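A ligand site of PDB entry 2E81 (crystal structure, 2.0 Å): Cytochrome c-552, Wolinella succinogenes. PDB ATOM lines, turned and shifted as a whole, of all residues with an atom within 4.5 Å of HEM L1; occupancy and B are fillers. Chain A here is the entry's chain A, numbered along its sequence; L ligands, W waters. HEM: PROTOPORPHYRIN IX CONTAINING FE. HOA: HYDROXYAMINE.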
ATOM      1  N   TYR A  74     -10.810 -15.539  11.920  1.00  0.00           N
ATOM      2  CA  TYR A  74     -12.170 -15.170  12.322  1.00  0.00           C
ATOM      3  C   TYR A  74     -12.139 -14.817  13.803  1.00  0.00           C
ATOM      4  O   TYR A  74     -11.924 -15.693  14.642  1.00  0.00           O
ATOM      5  CB  TYR A  74     -13.156 -16.317  12.085  1.00  0.00           C
ATOM      6  CG  TYR A  74     -14.534 -16.057  12.671  1.00  0.00           C
ATOM      7  CD1 TYR A  74     -15.307 -14.978  12.241  1.00  0.00           C
ATOM      8  CD2 TYR A  74     -15.061 -16.881  13.668  1.00  0.00           C
ATOM      9  CE1 TYR A  74     -16.576 -14.721  12.786  1.00  0.00           C
ATOM     10  CE2 TYR A  74     -16.320 -16.647  14.217  1.00  0.00           C
ATOM     11  CZ  TYR A  74     -17.071 -15.564  13.775  1.00  0.00           C
ATOM     12  OH  TYR A  74     -18.314 -15.332  14.319  1.00  0.00           O
ATOM     13  N   ASN A  75     -12.354 -13.544  14.116  1.00  0.00           N
ATOM     14  CA  ASN A  75     -12.338 -13.109  15.502  1.00  0.00           C
ATOM     15  C   ASN A  75     -13.702 -12.538  15.909  1.00  0.00           C
ATOM     16  O   ASN A  75     -14.541 -12.243  15.051  1.00  0.00           O
ATOM     17  CB  ASN A  75     -11.269 -12.027  15.700  1.00  0.00           C
ATOM     18  CG  ASN A  75      -9.932 -12.403  15.070  1.00  0.00           C
ATOM     19  OD1 ASN A  75      -9.348 -11.616  14.321  1.00  0.00           O
ATOM     20  ND2 ASN A  75      -9.443 -13.597  15.391  1.00  0.00           N
ATOM     21  N   ALA A  76     -13.913 -12.378  17.212  1.00  0.00           N
ATOM     22  CA  ALA A  76     -15.158 -11.829  17.710  1.00  0.00           C
ATOM     23  C   ALA A  76     -15.142 -10.346  17.333  1.00  0.00           C
ATOM     24  O   ALA A  76     -14.078  -9.787  17.074  1.00  0.00           O
ATOM     25  CB  ALA A  76     -15.244 -11.977  19.211  1.00  0.00           C
ATOM     26  N   PRO A  77     -16.312  -9.701  17.290  1.00  0.00           N
ATOM     27  CA  PRO A  77     -16.288  -8.288  16.935  1.00  0.00           C
ATOM     28  C   PRO A  77     -15.820  -7.432  18.091  1.00  0.00           C
ATOM     29  O   PRO A  77     -15.899  -7.829  19.249  1.00  0.00           O
ATOM     30  CB  PRO A  77     -17.735  -8.005  16.549  1.00  0.00           C
ATOM     31  CG  PRO A  77     -18.502  -8.901  17.463  1.00  0.00           C
ATOM     32  CD  PRO A  77     -17.695 -10.189  17.451  1.00  0.00           C
ATOM     33  N   ASP A  86      -9.703  -3.664  11.073  1.00  0.00           N
ATOM     34  CA  ASP A  86      -9.843  -5.119  11.188  1.00  0.00           C
ATOM     35  C   ASP A  86     -10.132  -5.722   9.824  1.00  0.00           C
ATOM     36  O   ASP A  86      -9.761  -6.858   9.540  1.00  0.00           O
ATOM     37  CB  ASP A  86     -10.936  -5.470  12.204  1.00  0.00           C
ATOM     38  CG  ASP A  86     -10.505  -5.217  13.633  1.00  0.00           C
ATOM     39  OD1 ASP A  86      -9.267  -5.174  13.879  1.00  0.00           O
ATOM     40  OD2 ASP A  86     -11.375  -5.065  14.512  1.00  0.00           O
ATOM     41  N   ASN A  87     -10.795  -4.936   8.968  1.00  0.00           N
ATOM     42  CA  ASN A  87     -11.120  -5.355   7.616  1.00  0.00           C
ATOM     43  C   ASN A  87      -9.796  -5.516   6.873  1.00  0.00           C
ATOM     44  O   ASN A  87      -9.614  -6.448   6.089  1.00  0.00           O
ATOM     45  CB  ASN A  87     -11.980  -4.278   6.942  1.00  0.00           C
ATOM     46  CG  ASN A  87     -12.510  -4.689   5.589  1.00  0.00           C
ATOM     47  OD1 ASN A  87     -12.356  -3.968   4.593  1.00  0.00           O
ATOM     48  ND2 ASN A  87     -13.152  -5.855   5.531  1.00  0.00           N
ATOM     49  N   THR A  90      -7.525  -8.628   8.879  1.00  0.00           N
ATOM     50  CA  THR A  90      -7.946 -10.014   8.754  1.00  0.00           C
ATOM     51  C   THR A  90      -7.225 -10.725   7.615  1.00  0.00           C
ATOM     52  O   THR A  90      -7.032 -10.163   6.539  1.00  0.00           O
ATOM     53  CB  THR A  90      -9.472 -10.157   8.548  1.00  0.00           C
ATOM     54  OG1 THR A  90      -9.805 -11.546   8.522  1.00  0.00           O
ATOM     55  CG2 THR A  90      -9.928  -9.499   7.244  1.00  0.00           C
ATOM     56  N   ARG A  92      -8.389 -12.901   5.924  1.00  0.00           N
ATOM     57  CA  ARG A  92      -9.360 -13.165   4.865  1.00  0.00           C
ATOM     58  C   ARG A  92      -9.185 -12.255   3.651  1.00  0.00           C
ATOM     59  O   ARG A  92      -9.407 -12.689   2.522  1.00  0.00           O
ATOM     60  CB  ARG A  92     -10.798 -13.070   5.413  1.00  0.00           C
ATOM     61  CG  ARG A  92     -11.075 -13.995   6.596  1.00  0.00           C
ATOM     62  CD  ARG A  92     -12.558 -14.382   6.737  1.00  0.00           C
ATOM     63  NE  ARG A  92     -13.454 -13.251   6.942  1.00  0.00           N
ATOM     64  CZ  ARG A  92     -13.694 -12.681   8.120  1.00  0.00           C
ATOM     65  NH1 ARG A  92     -13.097 -13.139   9.216  1.00  0.00           N
ATOM     66  NH2 ARG A  92     -14.531 -11.652   8.202  1.00  0.00           N
ATOM     67  N   THR A  93      -8.790 -10.998   3.857  1.00  0.00           N
ATOM     68  CA  THR A  93      -8.596 -10.091   2.732  1.00  0.00           C
ATOM     69  C   THR A  93      -7.250 -10.299   2.026  1.00  0.00           C
ATOM     70  O   THR A  93      -6.973  -9.682   1.005  1.00  0.00           O
ATOM     71  CB  THR A  93      -8.724  -8.611   3.159  1.00  0.00           C
ATOM     72  OG1 THR A  93      -7.969  -8.397   4.359  1.00  0.00           O
ATOM     73  CG2 THR A  93     -10.186  -8.243   3.368  1.00  0.00           C
ATOM     74  N   LEU A 104     -10.417 -10.987  -2.193  1.00  0.00           N
ATOM     75  CA  LEU A 104     -11.780 -10.478  -2.075  1.00  0.00           C
ATOM     76  C   LEU A 104     -12.137  -9.249  -2.914  1.00  0.00           C
ATOM     77  O   LEU A 104     -11.265  -8.491  -3.335  1.00  0.00           O
ATOM     78  CB  LEU A 104     -12.097 -10.230  -0.592  1.00  0.00           C
ATOM     79  CG  LEU A 104     -11.893 -11.498   0.263  1.00  0.00           C
ATOM     80  CD1 LEU A 104     -12.268 -11.226   1.722  1.00  0.00           C
ATOM     81  CD2 LEU A 104     -12.750 -12.632  -0.296  1.00  0.00           C
ATOM     82  N   ALA A 107     -16.840  -5.162  -2.443  1.00  0.00           N
ATOM     83  CA  ALA A 107     -17.971  -5.207  -1.526  1.00  0.00           C
ATOM     84  C   ALA A 107     -17.595  -5.403  -0.059  1.00  0.00           C
ATOM     85  O   ALA A 107     -18.395  -5.128   0.829  1.00  0.00           O
ATOM     86  CB  ALA A 107     -18.962  -6.294  -1.964  1.00  0.00           C
ATOM     87  N   CYS A 108     -16.376  -5.873   0.196  1.00  0.00           N
ATOM     88  CA  CYS A 108     -15.941  -6.080   1.575  1.00  0.00           C
ATOM     89  C   CYS A 108     -15.779  -4.807   2.392  1.00  0.00           C
ATOM     90  O   CYS A 108     -15.674  -4.870   3.621  1.00  0.00           O
ATOM     91  CB  CYS A 108     -14.656  -6.896   1.619  1.00  0.00           C
ATOM     92  SG  CYS A 108     -14.922  -8.668   1.365  1.00  0.00           S
ATOM     93  N   THR A 110     -18.034  -2.237   2.177  1.00  0.00           N
ATOM     94  CA  THR A 110     -19.405  -1.813   2.400  1.00  0.00           C
ATOM     95  C   THR A 110     -19.883  -1.466   3.797  1.00  0.00           C
ATOM     96  O   THR A 110     -20.444  -0.392   4.015  1.00  0.00           O
ATOM     97  CB  THR A 110     -20.396  -2.837   1.801  1.00  0.00           C
ATOM     98  OG1 THR A 110     -19.987  -3.147   0.460  1.00  0.00           O
ATOM     99  CG2 THR A 110     -21.806  -2.246   1.753  1.00  0.00           C
ATOM    100  N   CYS A 111     -19.674  -2.361   4.755  1.00  0.00           N
ATOM    101  CA  CYS A 111     -20.156  -2.128   6.110  1.00  0.00           C
ATOM    102  C   CYS A 111     -19.050  -1.768   7.079  1.00  0.00           C
ATOM    103  O   CYS A 111     -19.129  -2.097   8.268  1.00  0.00           O
ATOM    104  CB  CYS A 111     -20.903  -3.374   6.584  1.00  0.00           C
ATOM    105  SG  CYS A 111     -22.191  -3.955   5.426  1.00  0.00           S
ATOM    106  N   LYS A 112     -18.024  -1.078   6.595  1.00  0.00           N
ATOM    107  CA  LYS A 112     -16.903  -0.722   7.449  1.00  0.00           C
ATOM    108  C   LYS A 112     -16.564   0.759   7.469  1.00  0.00           C
ATOM    109  O   LYS A 112     -15.791   1.201   8.310  1.00  0.00           O
ATOM    110  CB  LYS A 112     -15.643  -1.477   6.982  1.00  0.00           C
ATOM    111  CG  LYS A 112     -15.786  -3.001   6.909  1.00  0.00           C
ATOM    112  CD  LYS A 112     -16.003  -3.588   8.302  1.00  0.00           C
ATOM    113  CE  LYS A 112     -16.036  -5.111   8.270  1.00  0.00           C
ATOM    114  NZ  LYS A 112     -17.283  -5.682   7.685  1.00  0.00           N
ATOM    115  N   TYR A 163     -29.266  -1.589  -0.689  1.00  0.00           N
ATOM    116  CA  TYR A 163     -29.626  -3.001  -0.539  1.00  0.00           C
ATOM    117  C   TYR A 163     -30.545  -3.304   0.642  1.00  0.00           C
ATOM    118  O   TYR A 163     -31.235  -4.327   0.643  1.00  0.00           O
ATOM    119  CB  TYR A 163     -28.361  -3.875  -0.469  1.00  0.00           C
ATOM    120  CG  TYR A 163     -27.415  -3.568   0.669  1.00  0.00           C
ATOM    121  CD1 TYR A 163     -27.732  -3.933   1.979  1.00  0.00           C
ATOM    122  CD2 TYR A 163     -26.195  -2.943   0.438  1.00  0.00           C
ATOM    123  CE1 TYR A 163     -26.843  -3.676   3.028  1.00  0.00           C
ATOM    124  CE2 TYR A 163     -25.308  -2.680   1.475  1.00  0.00           C
ATOM    125  CZ  TYR A 163     -25.637  -3.053   2.767  1.00  0.00           C
ATOM    126  OH  TYR A 163     -24.763  -2.782   3.802  1.00  0.00           O
ATOM    127  N   GLN A 191     -28.237  -1.948   8.430  1.00  0.00           N
ATOM    128  CA  GLN A 191     -27.523  -1.689   7.185  1.00  0.00           C
ATOM    129  C   GLN A 191     -26.342  -2.657   7.136  1.00  0.00           C
ATOM    130  O   GLN A 191     -25.925  -3.082   6.057  1.00  0.00           O
ATOM    131  CB  GLN A 191     -26.938  -0.275   7.169  1.00  0.00           C
ATOM    132  CG  GLN A 191     -27.930   0.844   7.318  1.00  0.00           C
ATOM    133  CD  GLN A 191     -27.218   2.181   7.319  1.00  0.00           C
ATOM    134  OE1 GLN A 191     -26.768   2.655   6.275  1.00  0.00           O
ATOM    135  NE2 GLN A 191     -27.081   2.774   8.491  1.00  0.00           N
ATOM    136  N   CYS A 192     -25.825  -3.004   8.300  1.00  0.00           N
ATOM    137  CA  CYS A 192     -24.662  -3.871   8.387  1.00  0.00           C
ATOM    138  C   CYS A 192     -24.846  -5.158   9.165  1.00  0.00           C
ATOM    139  O   CYS A 192     -24.309  -6.200   8.800  1.00  0.00           O
ATOM    140  CB  CYS A 192     -23.494  -3.089   8.989  1.00  0.00           C
ATOM    141  SG  CYS A 192     -23.213  -1.465   8.231  1.00  0.00           S
ATOM    142  N   HIS A 193     -25.586  -5.083  10.266  1.00  0.00           N
ATOM    143  CA  HIS A 193     -25.803  -6.240  11.117  1.00  0.00           C
ATOM    144  C   HIS A 193     -26.872  -7.192  10.615  1.00  0.00           C
ATOM    145  O   HIS A 193     -27.857  -7.463  11.303  1.00  0.00           O
ATOM    146  CB  HIS A 193     -26.109  -5.758  12.538  1.00  0.00           C
ATOM    147  CG  HIS A 193     -24.919  -5.213  13.258  1.00  0.00           C
ATOM    148  ND1 HIS A 193     -24.024  -5.985  13.983  1.00  0.00           N
ATOM    149  CD2 HIS A 193     -24.431  -3.944  13.316  1.00  0.00           C
ATOM    150  CE1 HIS A 193     -23.057  -5.172  14.436  1.00  0.00           C
ATOM    151  NE2 HIS A 193     -23.254  -3.924  14.070  1.00  0.00           N
ATOM    152  N   TYR A 196     -26.041 -11.691   4.469  1.00  0.00           N
ATOM    153  CA  TYR A 196     -26.028 -11.254   3.074  1.00  0.00           C
ATOM    154  C   TYR A 196     -25.209 -12.228   2.230  1.00  0.00           C
ATOM    155  O   TYR A 196     -24.582 -13.151   2.747  1.00  0.00           O
ATOM    156  CB  TYR A 196     -25.344  -9.890   2.983  1.00  0.00           C
ATOM    157  CG  TYR A 196     -23.841 -10.025   3.186  1.00  0.00           C
ATOM    158  CD1 TYR A 196     -23.296 -10.171   4.474  1.00  0.00           C
ATOM    159  CD2 TYR A 196     -22.976 -10.118   2.106  1.00  0.00           C
ATOM    160  CE1 TYR A 196     -21.932 -10.430   4.659  1.00  0.00           C
ATOM    161  CE2 TYR A 196     -21.615 -10.371   2.278  1.00  0.00           C
ATOM    162  CZ  TYR A 196     -21.103 -10.531   3.543  1.00  0.00           C
ATOM    163  OH  TYR A 196     -19.764 -10.820   3.696  1.00  0.00           O
ATOM    164  N   PHE A 198     -23.026 -12.133  -1.940  1.00  0.00           N
ATOM    165  CA  PHE A 198     -22.666 -11.303  -3.081  1.00  0.00           C
ATOM    166  C   PHE A 198     -23.285 -11.878  -4.338  1.00  0.00           C
ATOM    167  O   PHE A 198     -23.044 -13.036  -4.684  1.00  0.00           O
ATOM    168  CB  PHE A 198     -21.145 -11.229  -3.269  1.00  0.00           C
ATOM    169  CG  PHE A 198     -20.400 -10.578  -2.138  1.00  0.00           C
ATOM    170  CD1 PHE A 198     -20.968  -9.526  -1.415  1.00  0.00           C
ATOM    171  CD2 PHE A 198     -19.104 -10.976  -1.820  1.00  0.00           C
ATOM    172  CE1 PHE A 198     -20.265  -8.888  -0.407  1.00  0.00           C
ATOM    173  CE2 PHE A 198     -18.384 -10.341  -0.817  1.00  0.00           C
ATOM    174  CZ  PHE A 198     -18.964  -9.296  -0.110  1.00  0.00           C
ATOM    175  N   VAL A 216     -23.924  -6.650  -2.820  1.00  0.00           N
ATOM    176  CA  VAL A 216     -24.420  -7.099  -1.526  1.00  0.00           C
ATOM    177  C   VAL A 216     -25.917  -7.270  -1.655  1.00  0.00           C
ATOM    178  O   VAL A 216     -26.618  -6.334  -2.078  1.00  0.00           O
ATOM    179  CB  VAL A 216     -24.120  -6.058  -0.416  1.00  0.00           C
ATOM    180  CG1 VAL A 216     -24.877  -6.410   0.851  1.00  0.00           C
ATOM    181  CG2 VAL A 216     -22.627  -6.031  -0.138  1.00  0.00           C
ATOM    182  N   HIS A 255     -23.265 -12.835  10.592  1.00  0.00           N
ATOM    183  CA  HIS A 255     -23.919 -11.949  11.551  1.00  0.00           C
ATOM    184  C   HIS A 255     -25.356 -11.514  11.232  1.00  0.00           C
ATOM    185  O   HIS A 255     -25.591 -10.353  10.882  1.00  0.00           O
ATOM    186  CB  HIS A 255     -23.041 -10.718  11.746  1.00  0.00           C
ATOM    187  CG  HIS A 255     -22.499 -10.180  10.458  1.00  0.00           C
ATOM    188  ND1 HIS A 255     -23.311  -9.724   9.438  1.00  0.00           N
ATOM    189  CD2 HIS A 255     -21.225 -10.080  10.002  1.00  0.00           C
ATOM    190  CE1 HIS A 255     -22.558  -9.376   8.399  1.00  0.00           C
ATOM    191  NE2 HIS A 255     -21.292  -9.583   8.723  1.00  0.00           N
ATOM    192  N   ASP A 257     -27.632 -10.515  12.872  1.00  0.00           N
ATOM    193  CA  ASP A 257     -28.042  -9.908  14.136  1.00  0.00           C
ATOM    194  C   ASP A 257     -29.479  -9.392  14.138  1.00  0.00           C
ATOM    195  O   ASP A 257     -30.262  -9.714  15.037  1.00  0.00           O
ATOM    196  CB  ASP A 257     -27.090  -8.767  14.511  1.00  0.00           C
ATOM    197  CG  ASP A 257     -25.622  -9.195  14.486  1.00  0.00           C
ATOM    198  OD1 ASP A 257     -25.267 -10.164  15.182  1.00  0.00           O
ATOM    199  OD2 ASP A 257     -24.824  -8.557  13.758  1.00  0.00           O
ATOM    200  N   ALA A 376     -23.635 -17.151  14.333  1.00  0.00           N
ATOM    201  CA  ALA A 376     -22.939 -16.090  13.620  1.00  0.00           C
ATOM    202  C   ALA A 376     -23.249 -14.718  14.212  1.00  0.00           C
ATOM    203  O   ALA A 376     -22.451 -13.785  14.107  1.00  0.00           O
ATOM    204  CB  ALA A 376     -23.303 -16.113  12.138  1.00  0.00           C
ATOM    205  N   HIS A 378     -23.321 -12.960  17.353  1.00  0.00           N
ATOM    206  CA  HIS A 378     -22.814 -13.141  18.720  1.00  0.00           C
ATOM    207  C   HIS A 378     -23.755 -12.753  19.848  1.00  0.00           C
ATOM    208  O   HIS A 378     -23.569 -13.174  20.993  1.00  0.00           O
ATOM    209  CB  HIS A 378     -21.487 -12.395  18.869  1.00  0.00           C
ATOM    210  CG  HIS A 378     -20.392 -12.949  18.013  1.00  0.00           C
ATOM    211  ND1 HIS A 378     -19.644 -14.044  18.363  1.00  0.00           N
ATOM    212  CD2 HIS A 378     -19.947 -12.572  16.785  1.00  0.00           C
ATOM    213  CE1 HIS A 378     -18.786 -14.328  17.403  1.00  0.00           C
ATOM    214  NE2 HIS A 378     -18.945 -13.441  16.431  1.00  0.00           N
HETATM  215  CHA HEM L   1     -17.161  -7.841  11.205  1.00  0.00           C
HETATM  216  CHB HEM L   1     -14.444  -8.451   7.282  1.00  0.00           C
HETATM  217  CHC HEM L   1     -18.377  -8.057   4.513  1.00  0.00           C
HETATM  218  CHD HEM L   1     -20.760  -6.445   8.367  1.00  0.00           C
HETATM  219  C1A HEM L   1     -16.047  -8.018  10.389  1.00  0.00           C
HETATM  220  C2A HEM L   1     -14.686  -8.279  10.866  1.00  0.00           C
HETATM  221  C3A HEM L   1     -13.922  -8.409   9.751  1.00  0.00           C
HETATM  222  C4A HEM L   1     -14.806  -8.262   8.615  1.00  0.00           C
HETATM  223  CMA HEM L   1     -12.428  -8.722   9.693  1.00  0.00           C
HETATM  224  CAA HEM L   1     -14.220  -8.451  12.317  1.00  0.00           C
HETATM  225  CBA HEM L   1     -14.644  -9.812  12.884  1.00  0.00           C
HETATM  226  CGA HEM L   1     -13.952 -10.966  12.199  1.00  0.00           C
HETATM  227  O1A HEM L   1     -12.755 -11.213  12.496  1.00  0.00           O
HETATM  228  O2A HEM L   1     -14.585 -11.619  11.343  1.00  0.00           O
HETATM  229  C1B HEM L   1     -15.276  -8.421   6.177  1.00  0.00           C
HETATM  230  C2B HEM L   1     -14.880  -8.842   4.851  1.00  0.00           C
HETATM  231  C3B HEM L   1     -15.996  -8.808   4.069  1.00  0.00           C
HETATM  232  C4B HEM L   1     -17.068  -8.343   4.927  1.00  0.00           C
HETATM  233  CMB HEM L   1     -13.499  -9.276   4.408  1.00  0.00           C
HETATM  234  CAB HEM L   1     -16.061  -9.167   2.727  1.00  0.00           C
HETATM  235  CBB HEM L   1     -16.325 -10.511   2.406  1.00  0.00           C
HETATM  236  C1C HEM L   1     -19.398  -7.568   5.324  1.00  0.00           C
HETATM  237  C2C HEM L   1     -20.633  -7.000   4.832  1.00  0.00           C
HETATM  238  C3C HEM L   1     -21.284  -6.465   5.901  1.00  0.00           C
HETATM  239  C4C HEM L   1     -20.439  -6.748   7.055  1.00  0.00           C
HETATM  240  CMC HEM L   1     -21.099  -6.966   3.366  1.00  0.00           C
HETATM  241  CAC HEM L   1     -22.462  -5.715   5.883  1.00  0.00           C
HETATM  242  CBC HEM L   1     -23.642  -6.127   5.197  1.00  0.00           C
HETATM  243  C1D HEM L   1     -20.012  -6.737   9.483  1.00  0.00           C
HETATM  244  C2D HEM L   1     -20.512  -6.673  10.843  1.00  0.00           C
HETATM  245  C3D HEM L   1     -19.573  -7.246  11.641  1.00  0.00           C
HETATM  246  C4D HEM L   1     -18.436  -7.563  10.765  1.00  0.00           C
HETATM  247  CMD HEM L   1     -21.835  -6.089  11.326  1.00  0.00           C
HETATM  248  CAD HEM L   1     -19.687  -7.383  13.145  1.00  0.00           C
HETATM  249  CBD HEM L   1     -20.481  -8.503  13.820  1.00  0.00           C
HETATM  250  CGD HEM L   1     -19.822  -9.864  13.689  1.00  0.00           C
HETATM  251  O1D HEM L   1     -18.662  -9.924  13.233  1.00  0.00           O
HETATM  252  O2D HEM L   1     -20.459 -10.873  14.041  1.00  0.00           O
HETATM  253  NA  HEM L   1     -16.098  -8.009   9.013  1.00  0.00           N
HETATM  254  NB  HEM L   1     -16.613  -8.146   6.231  1.00  0.00           N
HETATM  255  NC  HEM L   1     -19.273  -7.378   6.687  1.00  0.00           N
HETATM  256  ND  HEM L   1     -18.747  -7.318   9.440  1.00  0.00           N
HETATM  257 FE   HEM L   1     -17.690  -7.771   7.832  1.00  0.00          FE
HETATM  258  N   HOA L   2     -18.145  -9.404   7.974  1.00  0.00           N
HETATM  259  O   HOA L   2     -17.248 -10.478   8.024  1.00  0.00           O
HETATM  260  CHA HEM L   3     -19.431  -4.235  15.904  1.00  0.00           C
HETATM  261  CHB HEM L   3     -23.777  -2.920  17.425  1.00  0.00           C
HETATM  262  CHC HEM L   3     -24.377  -0.202  13.572  1.00  0.00           C
HETATM  263  CHD HEM L   3     -20.658  -2.468  11.589  1.00  0.00           C
HETATM  264  C1A HEM L   3     -20.471  -3.910  16.754  1.00  0.00           C
HETATM  265  C2A HEM L   3     -20.604  -4.373  18.123  1.00  0.00           C
HETATM  266  C3A HEM L   3     -21.857  -4.053  18.519  1.00  0.00           C
HETATM  267  C4A HEM L   3     -22.486  -3.385  17.414  1.00  0.00           C
HETATM  268  CMA HEM L   3     -22.487  -4.305  19.884  1.00  0.00           C
HETATM  269  CAA HEM L   3     -19.515  -4.970  19.020  1.00  0.00           C
HETATM  270  CBA HEM L   3     -18.930  -3.894  19.935  1.00  0.00           C
HETATM  271  CGA HEM L   3     -17.843  -4.433  20.835  1.00  0.00           C
HETATM  272  O1A HEM L   3     -17.452  -5.611  20.669  1.00  0.00           O
HETATM  273  O2A HEM L   3     -17.354  -3.682  21.710  1.00  0.00           O
HETATM  274  C1B HEM L   3     -24.361  -2.104  16.488  1.00  0.00           C
HETATM  275  C2B HEM L   3     -25.620  -1.411  16.667  1.00  0.00           C
HETATM  276  C3B HEM L   3     -25.741  -0.525  15.662  1.00  0.00           C
HETATM  277  C4B HEM L   3     -24.571  -0.739  14.825  1.00  0.00           C
HETATM  278  CMB HEM L   3     -26.637  -1.670  17.779  1.00  0.00           C
HETATM  279  CAB HEM L   3     -26.797   0.382  15.476  1.00  0.00           C
HETATM  280  CBB HEM L   3     -27.010   1.457  16.378  1.00  0.00           C
HETATM  281  C1C HEM L   3     -23.374  -0.549  12.688  1.00  0.00           C
HETATM  282  C2C HEM L   3     -23.320  -0.098  11.323  1.00  0.00           C
HETATM  283  C3C HEM L   3     -22.326  -0.799  10.722  1.00  0.00           C
HETATM  284  C4C HEM L   3     -21.751  -1.645  11.751  1.00  0.00           C
HETATM  285  CMC HEM L   3     -24.239   0.903  10.627  1.00  0.00           C
HETATM  286  CAC HEM L   3     -21.996  -0.744   9.365  1.00  0.00           C
HETATM  287  CBC HEM L   3     -21.545   0.434   8.733  1.00  0.00           C
HETATM  288  C1D HEM L   3     -20.002  -3.184  12.579  1.00  0.00           C
HETATM  289  C2D HEM L   3     -18.695  -3.793  12.420  1.00  0.00           C
HETATM  290  C3D HEM L   3     -18.349  -4.310  13.623  1.00  0.00           C
HETATM  291  C4D HEM L   3     -19.417  -3.973  14.541  1.00  0.00           C
HETATM  292  CMD HEM L   3     -17.876  -3.859  11.141  1.00  0.00           C
HETATM  293  CAD HEM L   3     -17.066  -5.079  13.895  1.00  0.00           C
HETATM  294  CBD HEM L   3     -16.021  -4.143  14.474  1.00  0.00           C
HETATM  295  CGD HEM L   3     -14.645  -4.779  14.533  1.00  0.00           C
HETATM  296  O1D HEM L   3     -14.542  -5.918  15.048  1.00  0.00           O
HETATM  297  O2D HEM L   3     -13.676  -4.135  14.088  1.00  0.00           O
HETATM  298  NA  HEM L   3     -21.628  -3.253  16.342  1.00  0.00           N
HETATM  299  NB  HEM L   3     -23.715  -1.692  15.359  1.00  0.00           N
HETATM  300  NC  HEM L   3     -22.395  -1.486  12.956  1.00  0.00           N
HETATM  301  ND  HEM L   3     -20.420  -3.252  13.887  1.00  0.00           N
HETATM  302 FE   HEM L   3     -22.024  -2.413  14.640  1.00  0.00          FE
HETATM  303  O   HOH W   1     -22.553 -10.541  15.776  1.00  0.00           O
HETATM  304  O   HOH W   2     -10.490 -12.216  11.077  1.00  0.00           O
HETATM  305  O   HOH W   3     -17.332 -12.106  14.634  1.00  0.00           O
HETATM  306  O   HOH W   4     -15.973 -11.782   5.780  1.00  0.00           O
HETATM  307  O   HOH W   5     -19.973 -13.474  13.426  1.00  0.00           O
HETATM  308  O   HOH W   6     -18.004  -4.818   4.917  1.00  0.00           O
HETATM  309  O   HOH W   7     -10.985  -9.168  13.350  1.00  0.00           O
HETATM  310  O   HOH W   8     -17.356 -11.557  11.125  1.00  0.00           O
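Water W5 lies within hydrogen-bond range of O of Ala 376 (2.6 Å), OH of Tyr 74 (2.6 Å), O2D of HEM L1 (2.7 Å) and NE2 of His 378 (3.2 Å).
Water W8 bridges O2A of HEM L1 (2.8 Å) and O of HOA L2 (3.3 Å).
Water W7 bridges an oxygen (O1A) of HEM L1 (2.8 Å) and the side-chain amide oxygen (OD1) of Asn 75 (3.1 Å).
Water W2 lies within hydrogen-bond range of OG1 of Thr 90, O1A of HEM L1, NH1 of Arg 92, N of Tyr 74 and OD1 of Asn 75.
Water W3 lies within hydrogen-bond range of a ring nitrogen (NE2) of His 378 (2.8 Å), the backbone carbonyl oxygen of Asn 75 (2.8 Å), an oxygen (O1D) of HEM L1 (2.9 Å) and the side-chain hydroxyl of Tyr 74 (3.4 Å).
Water W4 lies within hydrogen-bond range of NH2 of Arg 92 and O of HOA L2.
ND1 of His 193 sits at hydrogen-bond distance from OD2 of Asp 257 (2.7 Å).
O of Asn 87 lies within hydrogen-bond range of OG1 of Thr 93.
The side-chain hydroxyl (OH) of Tyr 163 lies within hydrogen-bond range of the backbone carbonyl oxygen (O) of Gln 191, 2.6 Å away.
The side-chain hydroxyl of Tyr 74 is in hydrogen-bond range of a ring nitrogen (NE2) of His 378 (2.9 Å).
N of Arg 92 lies close to OG1 of Thr 90 (3.3 Å).
The backbone carbonyl oxygen (O) of Thr 90 is in hydrogen-bond range of the side-chain hydroxyl (OG1) of Thr 93, at 3.0 Å.
SG of Cys 111 is in hydrogen-bond range of OH of Tyr 163, 3.3 Å away.
The backbone carbonyl oxygen of Cys 108 lies within hydrogen-bond range of the side-chain amide nitrogen of Asn 87 (3.3 Å).
A nitrogen (N) of HOA L2 is bound to an iron atom (FE) of HEM L1 (1.7 Å).
NE2 of His 255 sits close to ND of HEM L1, at 3.5 Å.
Merely in contact with HEM L1: Tyr 74, Pro 77, Asp 86, Asn 87, Thr 90, Thr 93, Leu 104, Tyr 163, Gln 191, Cys 192, His 193, Tyr 196, Phe 198, Val 216, Ala 376 and His 378.
Of the 26 residues printed, 22 come within 4 Å of HEM L1.
The side-chain sulfur of Cys 108 is bonded to a carbon (CAB) of HEM L1.
O of HOA L2 sits at hydrogen-bond distance from NH2 of Arg 92 (3.0 Å).
N of HOA L2 lies close to NE2 of His 255 (3.2 Å).
SG of Cys 111 is bonded to CAC of HEM L1 (1.8 Å).
NH1 of Arg 92 is in salt-bridge range of O2A of HEM L1.
The side-chain sulfur (SG) of Cys 192 is covalently linked to a carbon (CAC) of HEM L3 (1.8 Å).
The side-chain carboxylate (OD2) of Asp 86 sits close to an oxygen (O2D) of HEM L3, 2.5 Å away.
The backbone NH (N) of Asn 75 is in hydrogen-bond range of an oxygen (O1A) of HEM L1.
A ring nitrogen (NE2) of His 193 is bound to an iron atom (FE) of HEM L3, 2.0 Å away.
NZ of Lys 112 is bound to FE of HEM L1, at 2.1 Å.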
